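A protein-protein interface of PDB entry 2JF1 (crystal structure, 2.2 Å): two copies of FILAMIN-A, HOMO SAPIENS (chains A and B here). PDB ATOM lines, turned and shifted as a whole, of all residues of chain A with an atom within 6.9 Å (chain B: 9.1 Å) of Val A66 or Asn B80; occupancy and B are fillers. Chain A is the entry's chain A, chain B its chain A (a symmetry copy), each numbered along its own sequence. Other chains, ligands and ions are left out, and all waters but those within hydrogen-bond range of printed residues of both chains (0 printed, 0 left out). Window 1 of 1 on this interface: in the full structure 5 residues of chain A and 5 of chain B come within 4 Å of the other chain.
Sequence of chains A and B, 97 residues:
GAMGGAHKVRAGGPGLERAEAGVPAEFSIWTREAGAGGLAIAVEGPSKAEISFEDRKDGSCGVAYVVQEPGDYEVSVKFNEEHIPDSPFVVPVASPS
O of Gly A22 lies within hydrogen-bond range of ND2 of Asn B80 (3.0 Å).
NE2 of Gln A68 is in hydrogen-bond range of OD1 of Asn B80 (3.0 Å).
The backbone NH (N) of Gly A22 sits at hydrogen-bond distance from the backbone carbonyl oxygen (O) of Val A67.
The backbone NH of Gln A68 is in hydrogen-bond range of the side-chain hydroxyl of Ser A47.
O of Glu A50 is in hydrogen-bond range of N of Val A66.
The backbone carbonyl oxygen (O) of Gly B38 sits at hydrogen-bond distance from the backbone NH (N) of Asn B80, at 2.7 Å.
O of Ala B36 touches O of Gly A22, 3.9 Å away.
Ala B36 touches Pro A24 (CB to CD, 3.6 Å).
Pro A24 touches Gly B37.
Gly B38 touches Glu A50 (CA to OE1, 3.7 Å).
CG2 of Val A66 touches C of Gly B37, 3.9 Å away.
Val A66 touches Gly B38.
Asn B80 touches Val A66.
Glu B81 touches Gln A68 (CG to CG, 3.0 Å).
Of chain B, only Gly B37 (3.9 Å), Gly B38 (3.6 Å) and Asn B80 (3.6 Å) come within 4 Å of Val A66.
Asn B80 touches three residues of chain A.
No residue of chain B comes within 4 Å of Val A67.
Of the printed residues of chain A, Glu B81 touches Gln A68 (3.0 Å).
Of the printed residues of chain A, Gly B38 touches Glu A50 and Val A66.
Ala A25 touches none of the printed residues of chain B.
Of the 18 printed residues of chain A, 5 touch a printed residue of chain B.
Hydrophobic or aromatic side chains of chain A that line the printed part of chain B: Pro A24 and Val A66.
Printed residues of chain B that touch a printed residue of chain A: Ala B36, Gly B37, Gly B38, Asn B80 and Glu B81.
Hydrophobic or aromatic side chains of chain B within 4 Å of the printed part of chain A: Ala B36.
Among the printed residues, no Asp or Glu carboxylate lies within 4 Å of a Lys or Arg side-chain nitrogen of the other chain.
No position is printed for both chains.
Of the 10 pairs that touch across the chains among the printed residues, none has its exchanged pair printed and touching as well.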
ATOM      1  N   GLU A  20      17.619  16.683  19.694  1.00  0.00           N
ATOM      2  CA  GLU A  20      17.540  17.982  19.070  1.00  0.00           C
ATOM      3  C   GLU A  20      17.377  18.927  20.227  1.00  0.00           C
ATOM      4  O   GLU A  20      16.565  18.681  21.130  1.00  0.00           O
ATOM      5  CB  GLU A  20      16.290  18.012  18.201  1.00  0.00           C
ATOM      6  CG  GLU A  20      16.233  19.059  17.168  1.00  0.00           C
ATOM      7  CD  GLU A  20      14.913  19.018  16.385  1.00  0.00           C
ATOM      8  OE1 GLU A  20      14.250  17.938  16.365  1.00  0.00           O
ATOM      9  OE2 GLU A  20      14.538  20.082  15.820  1.00  0.00           O
ATOM     10  N   ALA A  21      18.145  20.001  20.209  1.00  0.00           N
ATOM     11  CA  ALA A  21      18.097  21.058  21.225  1.00  0.00           C
ATOM     12  C   ALA A  21      16.689  21.629  21.397  1.00  0.00           C
ATOM     13  O   ALA A  21      16.048  22.028  20.431  1.00  0.00           O
ATOM     14  CB  ALA A  21      19.052  22.175  20.835  1.00  0.00           C
ATOM     15  N   GLY A  22      16.194  21.639  22.625  1.00  0.00           N
ATOM     16  CA  GLY A  22      14.862  22.144  22.866  1.00  0.00           C
ATOM     17  C   GLY A  22      13.744  21.113  22.655  1.00  0.00           C
ATOM     18  O   GLY A  22      12.611  21.392  22.930  1.00  0.00           O
ATOM     19  N   VAL A  23      14.057  19.935  22.162  1.00  0.00           N
ATOM     20  CA  VAL A  23      13.042  18.895  21.900  1.00  0.00           C
ATOM     21  C   VAL A  23      13.281  17.752  22.877  1.00  0.00           C
ATOM     22  O   VAL A  23      14.391  17.261  22.959  1.00  0.00           O
ATOM     23  CB  VAL A  23      13.118  18.369  20.422  1.00  0.00           C
ATOM     24  CG1 VAL A  23      11.983  17.336  20.113  1.00  0.00           C
ATOM     25  CG2 VAL A  23      13.003  19.549  19.427  1.00  0.00           C
ATOM     26  N   PRO A  24      12.251  17.348  23.643  1.00  0.00           N
ATOM     27  CA  PRO A  24      12.433  16.211  24.525  1.00  0.00           C
ATOM     28  C   PRO A  24      12.847  14.957  23.802  1.00  0.00           C
ATOM     29  O   PRO A  24      12.275  14.600  22.788  1.00  0.00           O
ATOM     30  CB  PRO A  24      11.064  16.053  25.206  1.00  0.00           C
ATOM     31  CG  PRO A  24      10.442  17.424  25.102  1.00  0.00           C
ATOM     32  CD  PRO A  24      10.925  17.972  23.808  1.00  0.00           C
ATOM     33  N   ALA A  25      13.895  14.349  24.351  1.00  0.00           N
ATOM     34  CA  ALA A  25      14.524  13.103  23.934  1.00  0.00           C
ATOM     35  C   ALA A  25      14.112  12.016  24.940  1.00  0.00           C
ATOM     36  O   ALA A  25      14.187  12.237  26.134  1.00  0.00           O
ATOM     37  CB  ALA A  25      16.052  13.268  23.891  1.00  0.00           C
ATOM     38  N   VAL A  43      23.092  13.666  32.477  1.00  0.00           N
ATOM     39  CA  VAL A  43      23.455  14.160  31.161  1.00  0.00           C
ATOM     40  C   VAL A  43      24.595  15.120  31.349  1.00  0.00           C
ATOM     41  O   VAL A  43      24.520  16.012  32.209  1.00  0.00           O
ATOM     42  CB  VAL A  43      22.275  14.874  30.479  1.00  0.00           C
ATOM     43  CG1 VAL A  43      22.690  15.405  29.118  1.00  0.00           C
ATOM     44  CG2 VAL A  43      21.097  13.916  30.354  1.00  0.00           C
ATOM     45  N   SER A  47      25.675  22.033  27.750  1.00  0.00           N
ATOM     46  CA  SER A  47      24.619  22.757  28.441  1.00  0.00           C
ATOM     47  C   SER A  47      23.926  21.861  29.442  1.00  0.00           C
ATOM     48  O   SER A  47      24.189  20.657  29.510  1.00  0.00           O
ATOM     49  CB  SER A  47      23.589  23.338  27.472  1.00  0.00           C
ATOM     50  OG  SER A  47      22.725  22.340  26.938  1.00  0.00           O
ATOM     51  N   LYS A  48      23.039  22.452  30.228  1.00  0.00           N
ATOM     52  CA  LYS A  48      22.343  21.742  31.259  1.00  0.00           C
ATOM     53  C   LYS A  48      21.087  21.093  30.693  1.00  0.00           C
ATOM     54  O   LYS A  48      20.466  21.617  29.763  1.00  0.00           O
ATOM     55  CB  LYS A  48      21.949  22.719  32.359  1.00  0.00           C
ATOM     56  CG  LYS A  48      22.937  22.825  33.490  1.00  0.00           C
ATOM     57  CD  LYS A  48      22.334  22.084  34.666  1.00  0.00           C
ATOM     58  CE  LYS A  48      23.283  21.875  35.819  1.00  0.00           C
ATOM     59  NZ  LYS A  48      22.544  21.164  36.915  1.00  0.00           N
ATOM     60  N   ALA A  49      20.674  19.986  31.296  1.00  0.00           N
ATOM     61  CA  ALA A  49      19.471  19.288  30.891  1.00  0.00           C
ATOM     62  C   ALA A  49      18.450  19.459  31.989  1.00  0.00           C
ATOM     63  O   ALA A  49      18.808  19.623  33.159  1.00  0.00           O
ATOM     64  CB  ALA A  49      19.777  17.764  30.697  1.00  0.00           C
ATOM     65  N   GLU A  50      17.191  19.432  31.594  1.00  0.00           N
ATOM     66  CA  GLU A  50      16.096  19.033  32.448  1.00  0.00           C
ATOM     67  C   GLU A  50      15.871  17.548  32.097  1.00  0.00           C
ATOM     68  O   GLU A  50      15.831  17.211  30.916  1.00  0.00           O
ATOM     69  CB  GLU A  50      14.810  19.789  32.070  1.00  0.00           C
ATOM     70  CG  GLU A  50      14.717  21.223  32.499  1.00  0.00           C
ATOM     71  CD  GLU A  50      14.828  22.189  31.363  1.00  0.00           C
ATOM     72  OE1 GLU A  50      15.228  21.777  30.244  1.00  0.00           O
ATOM     73  OE2 GLU A  50      14.532  23.374  31.602  1.00  0.00           O
ATOM     74  N   ILE A  51      15.708  16.706  33.121  1.00  0.00           N
ATOM     75  CA  ILE A  51      15.535  15.265  33.032  1.00  0.00           C
ATOM     76  C   ILE A  51      14.358  14.869  33.914  1.00  0.00           C
ATOM     77  O   ILE A  51      14.388  15.152  35.106  1.00  0.00           O
ATOM     78  CB  ILE A  51      16.791  14.492  33.590  1.00  0.00           C
ATOM     79  CG1 ILE A  51      18.095  15.082  33.037  1.00  0.00           C
ATOM     80  CG2 ILE A  51      16.673  12.997  33.320  1.00  0.00           C
ATOM     81  CD1 ILE A  51      19.378  14.779  33.774  1.00  0.00           C
ATOM     82  N   SER A  52      13.348  14.192  33.348  1.00  0.00           N
ATOM     83  CA  SER A  52      12.239  13.642  34.144  1.00  0.00           C
ATOM     84  C   SER A  52      12.091  12.145  34.004  1.00  0.00           C
ATOM     85  O   SER A  52      12.267  11.623  32.930  1.00  0.00           O
ATOM     86  CB  SER A  52      10.868  14.226  33.711  1.00  0.00           C
ATOM     87  OG  SER A  52      10.867  15.610  33.809  1.00  0.00           O
ATOM     88  N   ALA A  64      12.593  11.226  29.918  1.00  0.00           N
ATOM     89  CA  ALA A  64      12.594  12.272  28.927  1.00  0.00           C
ATOM     90  C   ALA A  64      13.597  13.314  29.436  1.00  0.00           C
ATOM     91  O   ALA A  64      13.632  13.579  30.630  1.00  0.00           O
ATOM     92  CB  ALA A  64      11.143  12.894  28.806  1.00  0.00           C
ATOM     93  N   TYR A  65      14.411  13.868  28.542  1.00  0.00           N
ATOM     94  CA  TYR A  65      15.342  14.942  28.883  1.00  0.00           C
ATOM     95  C   TYR A  65      15.379  15.974  27.746  1.00  0.00           C
ATOM     96  O   TYR A  65      15.105  15.641  26.559  1.00  0.00           O
ATOM     97  CB  TYR A  65      16.768  14.408  29.218  1.00  0.00           C
ATOM     98  CG  TYR A  65      17.537  13.875  28.007  1.00  0.00           C
ATOM     99  CD1 TYR A  65      18.354  14.718  27.254  1.00  0.00           C
ATOM    100  CD2 TYR A  65      17.434  12.520  27.615  1.00  0.00           C
ATOM    101  CE1 TYR A  65      19.043  14.266  26.133  1.00  0.00           C
ATOM    102  CE2 TYR A  65      18.152  12.027  26.499  1.00  0.00           C
ATOM    103  CZ  TYR A  65      18.937  12.912  25.753  1.00  0.00           C
ATOM    104  OH  TYR A  65      19.618  12.477  24.635  1.00  0.00           O
ATOM    105  N   VAL A  66      15.698  17.220  28.114  1.00  0.00           N
ATOM    106  CA  VAL A  66      15.851  18.330  27.149  1.00  0.00           C
ATOM    107  C   VAL A  66      17.163  19.024  27.451  1.00  0.00           C
ATOM    108  O   VAL A  66      17.447  19.275  28.604  1.00  0.00           O
ATOM    109  CB  VAL A  66      14.796  19.420  27.311  1.00  0.00           C
ATOM    110  CG1 VAL A  66      14.836  20.327  26.103  1.00  0.00           C
ATOM    111  CG2 VAL A  66      13.424  18.840  27.475  1.00  0.00           C
ATOM    112  N   VAL A  67      17.953  19.296  26.419  1.00  0.00           N
ATOM    113  CA  VAL A  67      19.158  20.114  26.526  1.00  0.00           C
ATOM    114  C   VAL A  67      18.879  21.310  25.621  1.00  0.00           C
ATOM    115  O   VAL A  67      18.023  21.219  24.735  1.00  0.00           O
ATOM    116  CB  VAL A  67      20.498  19.327  26.076  1.00  0.00           C
ATOM    117  CG1 VAL A  67      20.722  18.149  26.926  1.00  0.00           C
ATOM    118  CG2 VAL A  67      20.436  18.900  24.640  1.00  0.00           C
ATOM    119  N   GLN A  68      19.558  22.433  25.824  1.00  0.00           N
ATOM    120  CA  GLN A  68      19.184  23.656  25.063  1.00  0.00           C
ATOM    121  C   GLN A  68      20.152  24.017  23.949  1.00  0.00           C
ATOM    122  O   GLN A  68      19.814  24.808  23.063  1.00  0.00           O
ATOM    123  CB  GLN A  68      18.944  24.870  26.001  1.00  0.00           C
ATOM    124  CG  GLN A  68      17.748  24.689  26.996  1.00  0.00           C
ATOM    125  CD  GLN A  68      16.484  24.211  26.308  1.00  0.00           C
ATOM    126  OE1 GLN A  68      16.201  24.609  25.169  1.00  0.00           O
ATOM    127  NE2 GLN A  68      15.724  23.345  26.981  1.00  0.00           N
ATOM    128  N   GLY B   5       8.578  28.572  21.486  1.00  0.00           N
ATOM    129  CA  GLY B   5       7.189  28.172  21.925  1.00  0.00           C
ATOM    130  C   GLY B   5       6.871  28.482  23.387  1.00  0.00           C
ATOM    131  O   GLY B   5       5.831  28.067  23.883  1.00  0.00           O
ATOM    132  N   ALA B   6       7.770  29.203  24.061  1.00  0.00           N
ATOM    133  CA  ALA B   6       7.548  29.737  25.426  1.00  0.00           C
ATOM    134  C   ALA B   6       6.346  30.715  25.514  1.00  0.00           C
ATOM    135  O   ALA B   6       5.649  30.723  26.523  1.00  0.00           O
ATOM    136  CB  ALA B   6       8.767  30.385  25.912  1.00  0.00           C
ATOM    137  N   HIS B   7       6.088  31.507  24.454  1.00  0.00           N
ATOM    138  CA  HIS B   7       4.914  32.413  24.421  1.00  0.00           C
ATOM    139  C   HIS B   7       3.563  31.703  24.422  1.00  0.00           C
ATOM    140  O   HIS B   7       2.571  32.308  24.741  1.00  0.00           O
ATOM    141  CB  HIS B   7       4.950  33.482  23.315  1.00  0.00           C
ATOM    142  CG  HIS B   7       3.856  34.522  23.447  1.00  0.00           C
ATOM    143  ND1 HIS B   7       4.062  35.771  24.007  1.00  0.00           N
ATOM    144  CD2 HIS B   7       2.542  34.490  23.090  1.00  0.00           C
ATOM    145  CE1 HIS B   7       2.929  36.460  23.986  1.00  0.00           C
ATOM    146  NE2 HIS B   7       1.990  35.700  23.445  1.00  0.00           N
ATOM    147  N   VAL B   9       3.024  29.122  26.504  1.00  0.00           N
ATOM    148  CA  VAL B   9       2.773  28.667  27.858  1.00  0.00           C
ATOM    149  C   VAL B   9       2.251  29.846  28.680  1.00  0.00           C
ATOM    150  O   VAL B   9       2.780  30.938  28.587  1.00  0.00           O
ATOM    151  CB  VAL B   9       4.044  28.034  28.529  1.00  0.00           C
ATOM    152  CG1 VAL B   9       3.712  27.574  29.995  1.00  0.00           C
ATOM    153  CG2 VAL B   9       4.567  26.859  27.703  1.00  0.00           C
ATOM    154  N   GLY B  35       4.046  23.405  22.982  1.00  0.00           N
ATOM    155  CA  GLY B  35       4.717  22.245  22.454  1.00  0.00           C
ATOM    156  C   GLY B  35       5.365  21.458  23.572  1.00  0.00           C
ATOM    157  O   GLY B  35       5.083  21.659  24.745  1.00  0.00           O
ATOM    158  N   ALA B  36       6.251  20.547  23.197  1.00  0.00           N
ATOM    159  CA  ALA B  36       6.999  19.776  24.148  1.00  0.00           C
ATOM    160  C   ALA B  36       8.248  20.593  24.477  1.00  0.00           C
ATOM    161  O   ALA B  36       8.741  21.339  23.630  1.00  0.00           O
ATOM    162  CB  ALA B  36       7.362  18.494  23.506  1.00  0.00           C
ATOM    163  N   GLY B  37       8.760  20.484  25.691  1.00  0.00           N
ATOM    164  CA  GLY B  37       9.953  21.230  26.042  1.00  0.00           C
ATOM    165  C   GLY B  37      10.221  21.087  27.512  1.00  0.00           C
ATOM    166  O   GLY B  37       9.456  20.432  28.239  1.00  0.00           O
ATOM    167  N   GLY B  38      11.312  21.690  27.945  1.00  0.00           N
ATOM    168  CA  GLY B  38      11.636  21.763  29.357  1.00  0.00           C
ATOM    169  C   GLY B  38      10.989  22.997  30.007  1.00  0.00           C
ATOM    170  O   GLY B  38      11.119  24.129  29.487  1.00  0.00           O
ATOM    171  N   LEU B  39      10.327  22.726  31.147  1.00  0.00           N
ATOM    172  CA  LEU B  39       9.608  23.685  31.941  1.00  0.00           C
ATOM    173  C   LEU B  39      10.330  23.832  33.278  1.00  0.00           C
ATOM    174  O   LEU B  39      10.420  22.866  34.032  1.00  0.00           O
ATOM    175  CB  LEU B  39       8.154  23.211  32.135  1.00  0.00           C
ATOM    176  CG  LEU B  39       7.216  24.226  32.811  1.00  0.00           C
ATOM    177  CD1 LEU B  39       7.070  25.489  31.979  1.00  0.00           C
ATOM    178  CD2 LEU B  39       5.855  23.612  33.168  1.00  0.00           C
ATOM    179  N   ALA B  40      10.897  25.017  33.528  1.00  0.00           N
ATOM    180  CA  ALA B  40      11.519  25.295  34.805  1.00  0.00           C
ATOM    181  C   ALA B  40      10.816  26.400  35.617  1.00  0.00           C
ATOM    182  O   ALA B  40      10.455  27.456  35.073  1.00  0.00           O
ATOM    183  CB  ALA B  40      12.999  25.616  34.632  1.00  0.00           C
ATOM    184  N   VAL B  77       8.811  31.289  35.449  1.00  0.00           N
ATOM    185  CA  VAL B  77       8.398  30.104  34.742  1.00  0.00           C
ATOM    186  C   VAL B  77       9.012  30.293  33.371  1.00  0.00           C
ATOM    187  O   VAL B  77       8.760  31.291  32.691  1.00  0.00           O
ATOM    188  CB  VAL B  77       6.879  30.000  34.701  1.00  0.00           C
ATOM    189  CG1 VAL B  77       6.439  28.671  34.099  1.00  0.00           C
ATOM    190  CG2 VAL B  77       6.292  30.234  36.115  1.00  0.00           C
ATOM    191  N   LYS B  78       9.909  29.363  33.027  1.00  0.00           N
ATOM    192  CA  LYS B  78      10.699  29.406  31.791  1.00  0.00           C
ATOM    193  C   LYS B  78      10.465  28.126  31.019  1.00  0.00           C
ATOM    194  O   LYS B  78      10.408  27.039  31.619  1.00  0.00           O
ATOM    195  CB  LYS B  78      12.184  29.547  32.091  1.00  0.00           C
ATOM    196  CG  LYS B  78      12.541  30.895  32.676  1.00  0.00           C
ATOM    197  CD  LYS B  78      13.892  31.389  32.178  1.00  0.00           C
ATOM    198  CE  LYS B  78      14.824  31.440  33.291  1.00  0.00           C
ATOM    199  NZ  LYS B  78      16.013  32.257  32.916  1.00  0.00           N
ATOM    200  N   PHE B  79      10.289  28.259  29.708  1.00  0.00           N
ATOM    201  CA  PHE B  79      10.067  27.114  28.818  1.00  0.00           C
ATOM    202  C   PHE B  79      11.232  27.109  27.827  1.00  0.00           C
ATOM    203  O   PHE B  79      11.484  28.124  27.174  1.00  0.00           O
ATOM    204  CB  PHE B  79       8.680  27.201  28.142  1.00  0.00           C
ATOM    205  CG  PHE B  79       8.435  26.160  27.089  1.00  0.00           C
ATOM    206  CD1 PHE B  79       7.768  25.010  27.383  1.00  0.00           C
ATOM    207  CD2 PHE B  79       8.863  26.364  25.770  1.00  0.00           C
ATOM    208  CE1 PHE B  79       7.544  24.016  26.387  1.00  0.00           C
ATOM    209  CE2 PHE B  79       8.635  25.374  24.763  1.00  0.00           C
ATOM    210  CZ  PHE B  79       7.986  24.212  25.085  1.00  0.00           C
ATOM    211  N   ASN B  80      11.998  26.004  27.815  1.00  0.00           N
ATOM    212  CA  ASN B  80      13.311  25.933  27.119  1.00  0.00           C
ATOM    213  C   ASN B  80      14.136  27.196  27.361  1.00  0.00           C
ATOM    214  O   ASN B  80      14.591  27.868  26.407  1.00  0.00           O
ATOM    215  CB  ASN B  80      13.106  25.657  25.622  1.00  0.00           C
ATOM    216  CG  ASN B  80      12.612  24.232  25.366  1.00  0.00           C
ATOM    217  OD1 ASN B  80      12.832  23.347  26.191  1.00  0.00           O
ATOM    218  ND2 ASN B  80      11.945  24.011  24.245  1.00  0.00           N
ATOM    219  N   GLU B  81      14.257  27.557  28.641  1.00  0.00           N
ATOM    220  CA  GLU B  81      15.105  28.697  29.122  1.00  0.00           C
ATOM    221  C   GLU B  81      14.667  30.104  28.734  1.00  0.00           C
ATOM    222  O   GLU B  81      15.448  31.075  28.883  1.00  0.00           O
ATOM    223  CB  GLU B  81      16.565  28.517  28.691  1.00  0.00           C
ATOM    224  CG  GLU B  81      17.024  27.109  28.674  1.00  0.00           C
ATOM    225  CD  GLU B  81      17.744  26.641  29.907  1.00  0.00           C
ATOM    226  OE1 GLU B  81      18.988  26.406  29.790  1.00  0.00           O
ATOM    227  OE2 GLU B  81      17.070  26.455  30.961  1.00  0.00           O
ATOM    228  N   GLU B  82      13.435  30.234  28.230  1.00  0.00           N
ATOM    229  CA  GLU B  82      12.852  31.530  27.919  1.00  0.00           C
ATOM    230  C   GLU B  82      11.655  31.782  28.850  1.00  0.00           C
ATOM    231  O   GLU B  82      10.755  30.943  28.962  1.00  0.00           O
ATOM    232  CB  GLU B  82      12.379  31.539  26.461  1.00  0.00           C
ATOM    233  CG  GLU B  82      12.832  32.694  25.607  1.00  0.00           C
ATOM    234  CD  GLU B  82      14.344  32.725  25.328  1.00  0.00           C
ATOM    235  OE1 GLU B  82      14.905  31.679  24.947  1.00  0.00           O
ATOM    236  OE2 GLU B  82      14.964  33.815  25.462  1.00  0.00           O
ATOM    237  N   HIS B  83      11.640  32.955  29.487  1.00  0.00           N
ATOM    238  CA  HIS B  83      10.515  33.422  30.264  1.00  0.00           C
ATOM    239  C   HIS B  83       9.206  33.282  29.495  1.00  0.00           C
ATOM    240  O   HIS B  83       9.122  33.697  28.337  1.00  0.00           O
ATOM    241  CB  HIS B  83      10.772  34.879  30.665  1.00  0.00           C
ATOM    242  CG  HIS B  83      11.677  34.994  31.840  1.00  0.00           C
ATOM    243  ND1 HIS B  83      11.332  34.502  33.083  1.00  0.00           N
ATOM    244  CD2 HIS B  83      12.930  35.485  31.956  1.00  0.00           C
ATOM    245  CE1 HIS B  83      12.331  34.709  33.921  1.00  0.00           C
ATOM    246  NE2 HIS B  83      13.318  35.295  33.260  1.00  0.00           N
ATOM    247  N   ILE B  84       8.190  32.660  30.090  1.00  0.00           N
ATOM    248  CA  ILE B  84       6.821  32.660  29.460  1.00  0.00           C
ATOM    249  C   ILE B  84       6.247  34.115  29.564  1.00  0.00           C
ATOM    250  O   ILE B  84       6.910  34.969  30.219  1.00  0.00           O
ATOM    251  CB  ILE B  84       5.874  31.597  30.113  1.00  0.00           C
ATOM    252  CG1 ILE B  84       5.557  31.966  31.569  1.00  0.00           C
ATOM    253  CG2 ILE B  84       6.492  30.196  29.993  1.00  0.00           C
ATOM    254  CD1 ILE B  84       4.416  31.202  32.155  1.00  0.00           C
